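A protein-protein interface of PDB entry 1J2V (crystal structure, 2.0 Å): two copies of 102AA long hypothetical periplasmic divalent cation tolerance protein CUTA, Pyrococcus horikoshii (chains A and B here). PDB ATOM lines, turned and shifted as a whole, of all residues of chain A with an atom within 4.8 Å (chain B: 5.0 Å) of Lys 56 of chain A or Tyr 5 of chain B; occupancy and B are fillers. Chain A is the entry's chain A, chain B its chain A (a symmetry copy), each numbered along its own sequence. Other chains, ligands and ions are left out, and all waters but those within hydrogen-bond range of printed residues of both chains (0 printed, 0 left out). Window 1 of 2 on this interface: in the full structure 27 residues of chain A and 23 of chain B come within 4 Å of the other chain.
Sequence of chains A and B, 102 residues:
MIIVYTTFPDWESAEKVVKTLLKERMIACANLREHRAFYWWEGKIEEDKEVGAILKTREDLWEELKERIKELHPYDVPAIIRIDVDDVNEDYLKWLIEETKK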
ATOM      1  N   MET A   1      21.188  16.509 -10.706  1.00  0.00           N
ATOM      2  CA  MET A   1      21.789  16.056 -11.986  1.00  0.00           C
ATOM      3  C   MET A   1      23.304  16.031 -11.909  1.00  0.00           C
ATOM      4  O   MET A   1      23.916  16.550 -10.969  1.00  0.00           O
ATOM      5  CB  MET A   1      21.351  16.974 -13.133  1.00  0.00           C
ATOM      6  CG  MET A   1      21.830  18.420 -13.014  1.00  0.00           C
ATOM      7  SD  MET A   1      21.528  19.420 -14.502  1.00  0.00           S
ATOM      8  CE  MET A   1      22.905  18.936 -15.464  1.00  0.00           C
ATOM      9  N   ILE A   2      23.911  15.414 -12.909  1.00  0.00           N
ATOM     10  CA  ILE A   2      25.351  15.320 -12.943  1.00  0.00           C
ATOM     11  C   ILE A   2      25.909  15.544 -14.331  1.00  0.00           C
ATOM     12  O   ILE A   2      25.181  15.507 -15.315  1.00  0.00           O
ATOM     13  CB  ILE A   2      25.824  13.937 -12.447  1.00  0.00           C
ATOM     14  CG1 ILE A   2      25.298  12.845 -13.382  1.00  0.00           C
ATOM     15  CG2 ILE A   2      25.339  13.706 -11.039  1.00  0.00           C
ATOM     16  CD1 ILE A   2      26.037  11.527 -13.247  1.00  0.00           C
ATOM     17  N   ILE A   3      27.216  15.780 -14.375  1.00  0.00           N
ATOM     18  CA  ILE A   3      27.945  15.976 -15.610  1.00  0.00           C
ATOM     19  C   ILE A   3      28.908  14.831 -15.753  1.00  0.00           C
ATOM     20  O   ILE A   3      29.562  14.420 -14.803  1.00  0.00           O
ATOM     21  CB  ILE A   3      28.749  17.289 -15.611  1.00  0.00           C
ATOM     22  CG1 ILE A   3      27.787  18.478 -15.621  1.00  0.00           C
ATOM     23  CG2 ILE A   3      29.679  17.338 -16.819  1.00  0.00           C
ATOM     24  CD1 ILE A   3      26.762  18.421 -16.761  1.00  0.00           C
ATOM     25  N   ILE A  27      21.156   9.845 -21.537  1.00  0.00           N
ATOM     26  CA  ILE A  27      21.505  11.220 -21.249  1.00  0.00           C
ATOM     27  C   ILE A  27      20.507  12.067 -21.973  1.00  0.00           C
ATOM     28  O   ILE A  27      19.926  11.630 -22.969  1.00  0.00           O
ATOM     29  CB  ILE A  27      22.909  11.600 -21.791  1.00  0.00           C
ATOM     30  CG1 ILE A  27      22.911  11.554 -23.323  1.00  0.00           C
ATOM     31  CG2 ILE A  27      23.960  10.659 -21.217  1.00  0.00           C
ATOM     32  CD1 ILE A  27      24.107  12.155 -23.984  1.00  0.00           C
ATOM     33  N   ALA A  28      20.323  13.291 -21.499  1.00  0.00           N
ATOM     34  CA  ALA A  28      19.389  14.229 -22.129  1.00  0.00           C
ATOM     35  C   ALA A  28      20.096  15.053 -23.186  1.00  0.00           C
ATOM     36  O   ALA A  28      19.606  15.186 -24.307  1.00  0.00           O
ATOM     37  CB  ALA A  28      18.801  15.158 -21.082  1.00  0.00           C
ATOM     38  N   CYS A  29      21.282  15.550 -22.836  1.00  0.00           N
ATOM     39  CA  CYS A  29      22.041  16.407 -23.748  1.00  0.00           C
ATOM     40  C   CYS A  29      23.560  16.180 -23.739  1.00  0.00           C
ATOM     41  O   CYS A  29      24.128  15.676 -22.752  1.00  0.00           O
ATOM     42  CB  CYS A  29      21.740  17.859 -23.390  1.00  0.00           C
ATOM     43  SG  CYS A  29      22.619  19.101 -24.282  1.00  0.00           S
ATOM     44  N   ASN A  31      27.401  18.084 -25.267  1.00  0.00           N
ATOM     45  CA  ASN A  31      28.077  19.223 -25.875  1.00  0.00           C
ATOM     46  C   ASN A  31      29.479  18.752 -26.222  1.00  0.00           C
ATOM     47  O   ASN A  31      30.270  18.464 -25.332  1.00  0.00           O
ATOM     48  CB  ASN A  31      28.170  20.401 -24.906  1.00  0.00           C
ATOM     49  CG  ASN A  31      26.825  21.050 -24.629  1.00  0.00           C
ATOM     50  OD1 ASN A  31      26.647  21.753 -23.630  1.00  0.00           O
ATOM     51  ND2 ASN A  31      25.863  20.796 -25.505  1.00  0.00           N
ATOM     52  N   ILE A  54      30.641  16.651 -23.108  1.00  0.00           N
ATOM     53  CA  ILE A  54      30.010  16.965 -21.842  1.00  0.00           C
ATOM     54  C   ILE A  54      28.598  16.384 -21.910  1.00  0.00           C
ATOM     55  O   ILE A  54      27.726  16.910 -22.623  1.00  0.00           O
ATOM     56  CB  ILE A  54      29.888  18.477 -21.614  1.00  0.00           C
ATOM     57  CG1 ILE A  54      31.274  19.113 -21.641  1.00  0.00           C
ATOM     58  CG2 ILE A  54      29.234  18.751 -20.270  1.00  0.00           C
ATOM     59  CD1 ILE A  54      31.281  20.596 -21.436  1.00  0.00           C
ATOM     60  N   LEU A  55      28.390  15.284 -21.189  1.00  0.00           N
ATOM     61  CA  LEU A  55      27.095  14.609 -21.135  1.00  0.00           C
ATOM     62  C   LEU A  55      26.371  15.063 -19.885  1.00  0.00           C
ATOM     63  O   LEU A  55      26.984  15.240 -18.836  1.00  0.00           O
ATOM     64  CB  LEU A  55      27.288  13.093 -21.070  1.00  0.00           C
ATOM     65  CG  LEU A  55      28.275  12.624 -22.125  1.00  0.00           C
ATOM     66  CD1 LEU A  55      28.560  11.134 -21.940  1.00  0.00           C
ATOM     67  CD2 LEU A  55      27.707  12.930 -23.503  1.00  0.00           C
ATOM     68  N   LYS A  56      25.064  15.240 -19.986  1.00  0.00           N
ATOM     69  CA  LYS A  56      24.289  15.679 -18.840  1.00  0.00           C
ATOM     70  C   LYS A  56      23.096  14.759 -18.615  1.00  0.00           C
ATOM     71  O   LYS A  56      22.243  14.618 -19.494  1.00  0.00           O
ATOM     72  CB  LYS A  56      23.804  17.102 -19.074  1.00  0.00           C
ATOM     73  CG  LYS A  56      24.850  17.987 -19.717  1.00  0.00           C
ATOM     74  CD  LYS A  56      24.269  19.329 -20.091  1.00  0.00           C
ATOM     75  CE  LYS A  56      25.278  20.157 -20.869  1.00  0.00           C
ATOM     76  NZ  LYS A  56      24.615  21.334 -21.451  1.00  0.00           N
ATOM     77  N   THR A  57      23.041  14.124 -17.445  1.00  0.00           N
ATOM     78  CA  THR A  57      21.918  13.246 -17.121  1.00  0.00           C
ATOM     79  C   THR A  57      21.590  13.163 -15.621  1.00  0.00           C
ATOM     80  O   THR A  57      22.027  14.027 -14.821  1.00  0.00           O
ATOM     81  CB  THR A  57      22.142  11.828 -17.693  1.00  0.00           C
ATOM     82  OG1 THR A  57      20.908  11.108 -17.658  1.00  0.00           O
ATOM     83  CG2 THR A  57      23.179  11.068 -16.907  1.00  0.00           C
ATOM     84  N   TYR A  92      14.714  23.458 -16.556  1.00  0.00           N
ATOM     85  CA  TYR A  92      15.737  22.586 -17.156  1.00  0.00           C
ATOM     86  C   TYR A  92      15.824  21.152 -16.691  1.00  0.00           C
ATOM     87  O   TYR A  92      15.813  20.196 -17.501  1.00  0.00           O
ATOM     88  CB  TYR A  92      17.091  23.291 -17.076  1.00  0.00           C
ATOM     89  CG  TYR A  92      18.164  22.615 -17.840  1.00  0.00           C
ATOM     90  CD1 TYR A  92      18.198  22.651 -19.244  1.00  0.00           C
ATOM     91  CD2 TYR A  92      19.168  21.931 -17.155  1.00  0.00           C
ATOM     92  CE1 TYR A  92      19.230  22.010 -19.939  1.00  0.00           C
ATOM     93  CE2 TYR A  92      20.184  21.279 -17.843  1.00  0.00           C
ATOM     94  CZ  TYR A  92      20.213  21.321 -19.232  1.00  0.00           C
ATOM     95  OH  TYR A  92      21.215  20.669 -19.915  1.00  0.00           O
ATOM     96  N   LEU A  96      15.101  17.585 -18.325  1.00  0.00           N
ATOM     97  CA  LEU A  96      16.100  16.520 -18.336  1.00  0.00           C
ATOM     98  C   LEU A  96      15.539  15.222 -17.768  1.00  0.00           C
ATOM     99  O   LEU A  96      15.893  14.129 -18.236  1.00  0.00           O
ATOM    100  CB  LEU A  96      17.341  16.962 -17.539  1.00  0.00           C
ATOM    101  CG  LEU A  96      18.551  16.012 -17.401  1.00  0.00           C
ATOM    102  CD1 LEU A  96      19.758  16.830 -16.970  1.00  0.00           C
ATOM    103  CD2 LEU A  96      18.251  14.922 -16.382  1.00  0.00           C
ATOM    104  N   ILE B   3      31.129  27.877 -10.210  1.00  0.00           N
ATOM    105  CA  ILE B   3      31.106  27.941 -11.655  1.00  0.00           C
ATOM    106  C   ILE B   3      29.677  27.776 -12.092  1.00  0.00           C
ATOM    107  O   ILE B   3      28.943  26.942 -11.579  1.00  0.00           O
ATOM    108  CB  ILE B   3      31.943  26.822 -12.303  1.00  0.00           C
ATOM    109  CG1 ILE B   3      33.425  27.053 -12.001  1.00  0.00           C
ATOM    110  CG2 ILE B   3      31.699  26.784 -13.808  1.00  0.00           C
ATOM    111  CD1 ILE B   3      33.915  28.452 -12.396  1.00  0.00           C
ATOM    112  N   VAL B   4      29.283  28.603 -13.039  1.00  0.00           N
ATOM    113  CA  VAL B   4      27.948  28.563 -13.581  1.00  0.00           C
ATOM    114  C   VAL B   4      28.092  28.390 -15.081  1.00  0.00           C
ATOM    115  O   VAL B   4      28.687  29.222 -15.769  1.00  0.00           O
ATOM    116  CB  VAL B   4      27.189  29.859 -13.251  1.00  0.00           C
ATOM    117  CG1 VAL B   4      25.742  29.795 -13.785  1.00  0.00           C
ATOM    118  CG2 VAL B   4      27.194  30.063 -11.735  1.00  0.00           C
ATOM    119  N   TYR B   5      27.582  27.273 -15.577  1.00  0.00           N
ATOM    120  CA  TYR B   5      27.650  26.959 -16.996  1.00  0.00           C
ATOM    121  C   TYR B   5      26.272  27.098 -17.652  1.00  0.00           C
ATOM    122  O   TYR B   5      25.275  26.566 -17.145  1.00  0.00           O
ATOM    123  CB  TYR B   5      28.139  25.524 -17.162  1.00  0.00           C
ATOM    124  CG  TYR B   5      28.221  25.091 -18.606  1.00  0.00           C
ATOM    125  CD1 TYR B   5      29.018  25.795 -19.506  1.00  0.00           C
ATOM    126  CD2 TYR B   5      27.528  23.972 -19.071  1.00  0.00           C
ATOM    127  CE1 TYR B   5      29.145  25.383 -20.834  1.00  0.00           C
ATOM    128  CE2 TYR B   5      27.627  23.568 -20.393  1.00  0.00           C
ATOM    129  CZ  TYR B   5      28.442  24.267 -21.269  1.00  0.00           C
ATOM    130  OH  TYR B   5      28.559  23.847 -22.579  1.00  0.00           O
ATOM    131  N   THR B   6      26.222  27.880 -18.737  1.00  0.00           N
ATOM    132  CA  THR B   6      25.008  28.091 -19.522  1.00  0.00           C
ATOM    133  C   THR B   6      25.396  28.143 -20.990  1.00  0.00           C
ATOM    134  O   THR B   6      26.539  28.486 -21.332  1.00  0.00           O
ATOM    135  CB  THR B   6      24.283  29.415 -19.191  1.00  0.00           C
ATOM    136  OG1 THR B   6      23.076  29.514 -19.970  1.00  0.00           O
ATOM    137  CG2 THR B   6      25.193  30.622 -19.510  1.00  0.00           C
ATOM    138  N   THR B   7      24.447  27.818 -21.862  1.00  0.00           N
ATOM    139  CA  THR B   7      24.722  27.784 -23.294  1.00  0.00           C
ATOM    140  C   THR B   7      23.898  28.825 -24.047  1.00  0.00           C
ATOM    141  O   THR B   7      22.794  29.179 -23.623  1.00  0.00           O
ATOM    142  CB  THR B   7      24.396  26.396 -23.853  1.00  0.00           C
ATOM    143  OG1 THR B   7      25.096  25.393 -23.098  1.00  0.00           O
ATOM    144  CG2 THR B   7      24.804  26.321 -25.295  1.00  0.00           C
ATOM    145  N   ARG B  33      33.033  29.699 -25.499  1.00  0.00           N
ATOM    146  CA  ARG B  33      33.632  28.914 -26.556  1.00  0.00           C
ATOM    147  C   ARG B  33      32.521  28.088 -27.186  1.00  0.00           C
ATOM    148  O   ARG B  33      31.661  27.554 -26.499  1.00  0.00           O
ATOM    149  CB  ARG B  33      34.786  28.028 -26.018  1.00  0.00           C
ATOM    150  CG  ARG B  33      34.423  26.607 -25.516  1.00  0.00           C
ATOM    151  CD  ARG B  33      33.967  26.615 -24.079  1.00  0.00           C
ATOM    152  NE  ARG B  33      33.404  25.339 -23.643  1.00  0.00           N
ATOM    153  CZ  ARG B  33      32.204  24.874 -23.995  1.00  0.00           C
ATOM    154  NH1 ARG B  33      31.417  25.567 -24.808  1.00  0.00           N
ATOM    155  NH2 ARG B  33      31.765  23.731 -23.492  1.00  0.00           N
ATOM    156  N   HIS B  35      30.557  25.044 -29.295  1.00  0.00           N
ATOM    157  CA  HIS B  35      30.497  23.580 -29.126  1.00  0.00           C
ATOM    158  C   HIS B  35      29.287  23.100 -29.905  1.00  0.00           C
ATOM    159  O   HIS B  35      28.368  23.881 -30.155  1.00  0.00           O
ATOM    160  CB  HIS B  35      30.396  23.119 -27.657  1.00  0.00           C
ATOM    161  CG  HIS B  35      29.166  23.586 -26.946  1.00  0.00           C
ATOM    162  ND1 HIS B  35      29.200  24.499 -25.923  1.00  0.00           N
ATOM    163  CD2 HIS B  35      27.884  23.218 -27.123  1.00  0.00           C
ATOM    164  CE1 HIS B  35      27.954  24.680 -25.486  1.00  0.00           C
ATOM    165  NE2 HIS B  35      27.150  23.923 -26.191  1.00  0.00           N
ATOM    166  N   GLY B  52      28.843  27.956 -25.548  1.00  0.00           N
ATOM    167  CA  GLY B  52      28.783  27.659 -24.132  1.00  0.00           C
ATOM    168  C   GLY B  52      29.531  28.701 -23.344  1.00  0.00           C
ATOM    169  O   GLY B  52      30.508  29.249 -23.829  1.00  0.00           O
ATOM    170  N   ALA B  53      29.072  28.979 -22.133  1.00  0.00           N
ATOM    171  CA  ALA B  53      29.724  29.979 -21.305  1.00  0.00           C
ATOM    172  C   ALA B  53      30.048  29.463 -19.907  1.00  0.00           C
ATOM    173  O   ALA B  53      29.257  28.754 -19.303  1.00  0.00           O
ATOM    174  CB  ALA B  53      28.846  31.251 -21.217  1.00  0.00           C
ATOM    175  N   ILE B  54      31.240  29.803 -19.431  1.00  0.00           N
ATOM    176  CA  ILE B  54      31.678  29.445 -18.096  1.00  0.00           C
ATOM    177  C   ILE B  54      31.766  30.751 -17.307  1.00  0.00           C
ATOM    178  O   ILE B  54      32.677  31.569 -17.527  1.00  0.00           O
ATOM    179  CB  ILE B  54      33.069  28.799 -18.097  1.00  0.00           C
ATOM    180  CG1 ILE B  54      33.051  27.542 -18.960  1.00  0.00           C
ATOM    181  CG2 ILE B  54      33.473  28.431 -16.678  1.00  0.00           C
ATOM    182  CD1 ILE B  54      34.363  26.826 -19.042  1.00  0.00           C
ATOM    183  N   LEU B  55      30.800  30.953 -16.413  1.00  0.00           N
ATOM    184  CA  LEU B  55      30.742  32.144 -15.569  1.00  0.00           C
ATOM    185  C   LEU B  55      31.346  31.805 -14.223  1.00  0.00           C
ATOM    186  O   LEU B  55      31.148  30.710 -13.705  1.00  0.00           O
ATOM    187  CB  LEU B  55      29.290  32.579 -15.362  1.00  0.00           C
ATOM    188  CG  LEU B  55      28.542  32.623 -16.684  1.00  0.00           C
ATOM    189  CD1 LEU B  55      27.064  32.916 -16.430  1.00  0.00           C
ATOM    190  CD2 LEU B  55      29.185  33.671 -17.580  1.00  0.00           C
ATOM    191  N   ALA B  79      19.985  26.691 -19.599  1.00  0.00           N
ATOM    192  CA  ALA B  79      20.565  25.637 -18.765  1.00  0.00           C
ATOM    193  C   ALA B  79      21.414  26.547 -17.891  1.00  0.00           C
ATOM    194  O   ALA B  79      22.231  27.350 -18.406  1.00  0.00           O
ATOM    195  CB  ALA B  79      21.448  24.707 -19.538  1.00  0.00           C
ATOM    196  N   ILE B  80      21.190  26.483 -16.584  1.00  0.00           N
ATOM    197  CA  ILE B  80      21.927  27.308 -15.612  1.00  0.00           C
ATOM    198  C   ILE B  80      22.397  26.249 -14.601  1.00  0.00           C
ATOM    199  O   ILE B  80      21.626  25.809 -13.708  1.00  0.00           O
ATOM    200  CB  ILE B  80      21.007  28.317 -14.909  1.00  0.00           C
ATOM    201  CG1 ILE B  80      20.355  29.202 -15.963  1.00  0.00           C
ATOM    202  CG2 ILE B  80      21.808  29.159 -13.932  1.00  0.00           C
ATOM    203  CD1 ILE B  80      19.189  30.021 -15.433  1.00  0.00           C
ATOM    204  N   ILE B  81      23.650  25.815 -14.775  1.00  0.00           N
ATOM    205  CA  ILE B  81      24.245  24.782 -13.965  1.00  0.00           C
ATOM    206  C   ILE B  81      25.338  25.329 -13.048  1.00  0.00           C
ATOM    207  O   ILE B  81      26.295  25.960 -13.495  1.00  0.00           O
ATOM    208  CB  ILE B  81      24.784  23.667 -14.903  1.00  0.00           C
ATOM    209  CG1 ILE B  81      23.617  23.053 -15.688  1.00  0.00           C
ATOM    210  CG2 ILE B  81      25.490  22.581 -14.106  1.00  0.00           C
ATOM    211  CD1 ILE B  81      24.031  22.183 -16.844  1.00  0.00           C
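3 positions are printed for both chains. Of the 7 pairs that touch across the chains among the printed residues, none has its exchanged pair printed and touching as well.
A ring nitrogen (NE2) of His 35 of chain B sits close to the side-chain amide oxygen (OD1) of Asn 31 of chain A. The side-chain hydroxyl of Tyr 5 of chain B is in hydrogen-bond range of the side-chain amide oxygen of Asn 31 of chain A (3.0 Å).
Of the 13 printed residues of chain A, 5 touch a printed residue of chain B. Hydrophobic or aromatic side chains of chain B that line the printed part of chain A: Tyr 5, His 35, Ala 79 and Ile 81. Among the printed residues, 7 pairs touch across the chains.
Of chain A, only Asn 31 and Lys 56 come within 4 Å of Tyr 5 of chain B. Printed residues of chain A within 4 Å of Ile 81 of chain B: Met 1. Printed residues of chain A within 4 Å of Ala 79 of chain B: Tyr 92 (3.5 Å). Printed residues of chain B within 4 Å of Ile 54 of chain A: Arg 33. Printed residues of chain A within 4 Å of His 35 of chain B: Asn 31. Leu 96 of chain A touches none of the printed residues of chain B. The nearest printed residue of chain B that does not touch Met 1 of chain A is Ile 80 of chain B (6.4 Å).
CE of Met 1 of chain A touches CD1 of Ile 81 of chain B, at 3.7 Å. Thr 7 of chain B touches Asn 31 of chain A (OG1 to OD1, 3.99 Å). Ile 54 of chain A touches Arg 33 of chain B. Lys 56 of chain A touches Tyr 5 of chain B. Tyr 92 of chain A touches Ala 79 of chain B.
OD1 of Asn 31 of chain A is in hydrogen-bond range of NZ of Lys 56 of chain A. The backbone NH of Ala 28 of chain A is in hydrogen-bond range of the backbone carbonyl oxygen of Lys 56 of chain A. The backbone NH (N) of Tyr 5 of chain B lies within hydrogen-bond range of the backbone carbonyl oxygen (O) of Ile 81 of chain B (2.8 Å). OH of Tyr 5 of chain B is in hydrogen-bond range of NH2 of Arg 33 of chain B (3.3 Å). OH of Tyr 5 of chain B sits close to ND1 of His 35 of chain B, 3.5 Å away. The backbone carbonyl oxygen (O) of Asn 31 of chain A sits at hydrogen-bond distance from the backbone NH (N) of Ile 54 of chain A (2.9 Å).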
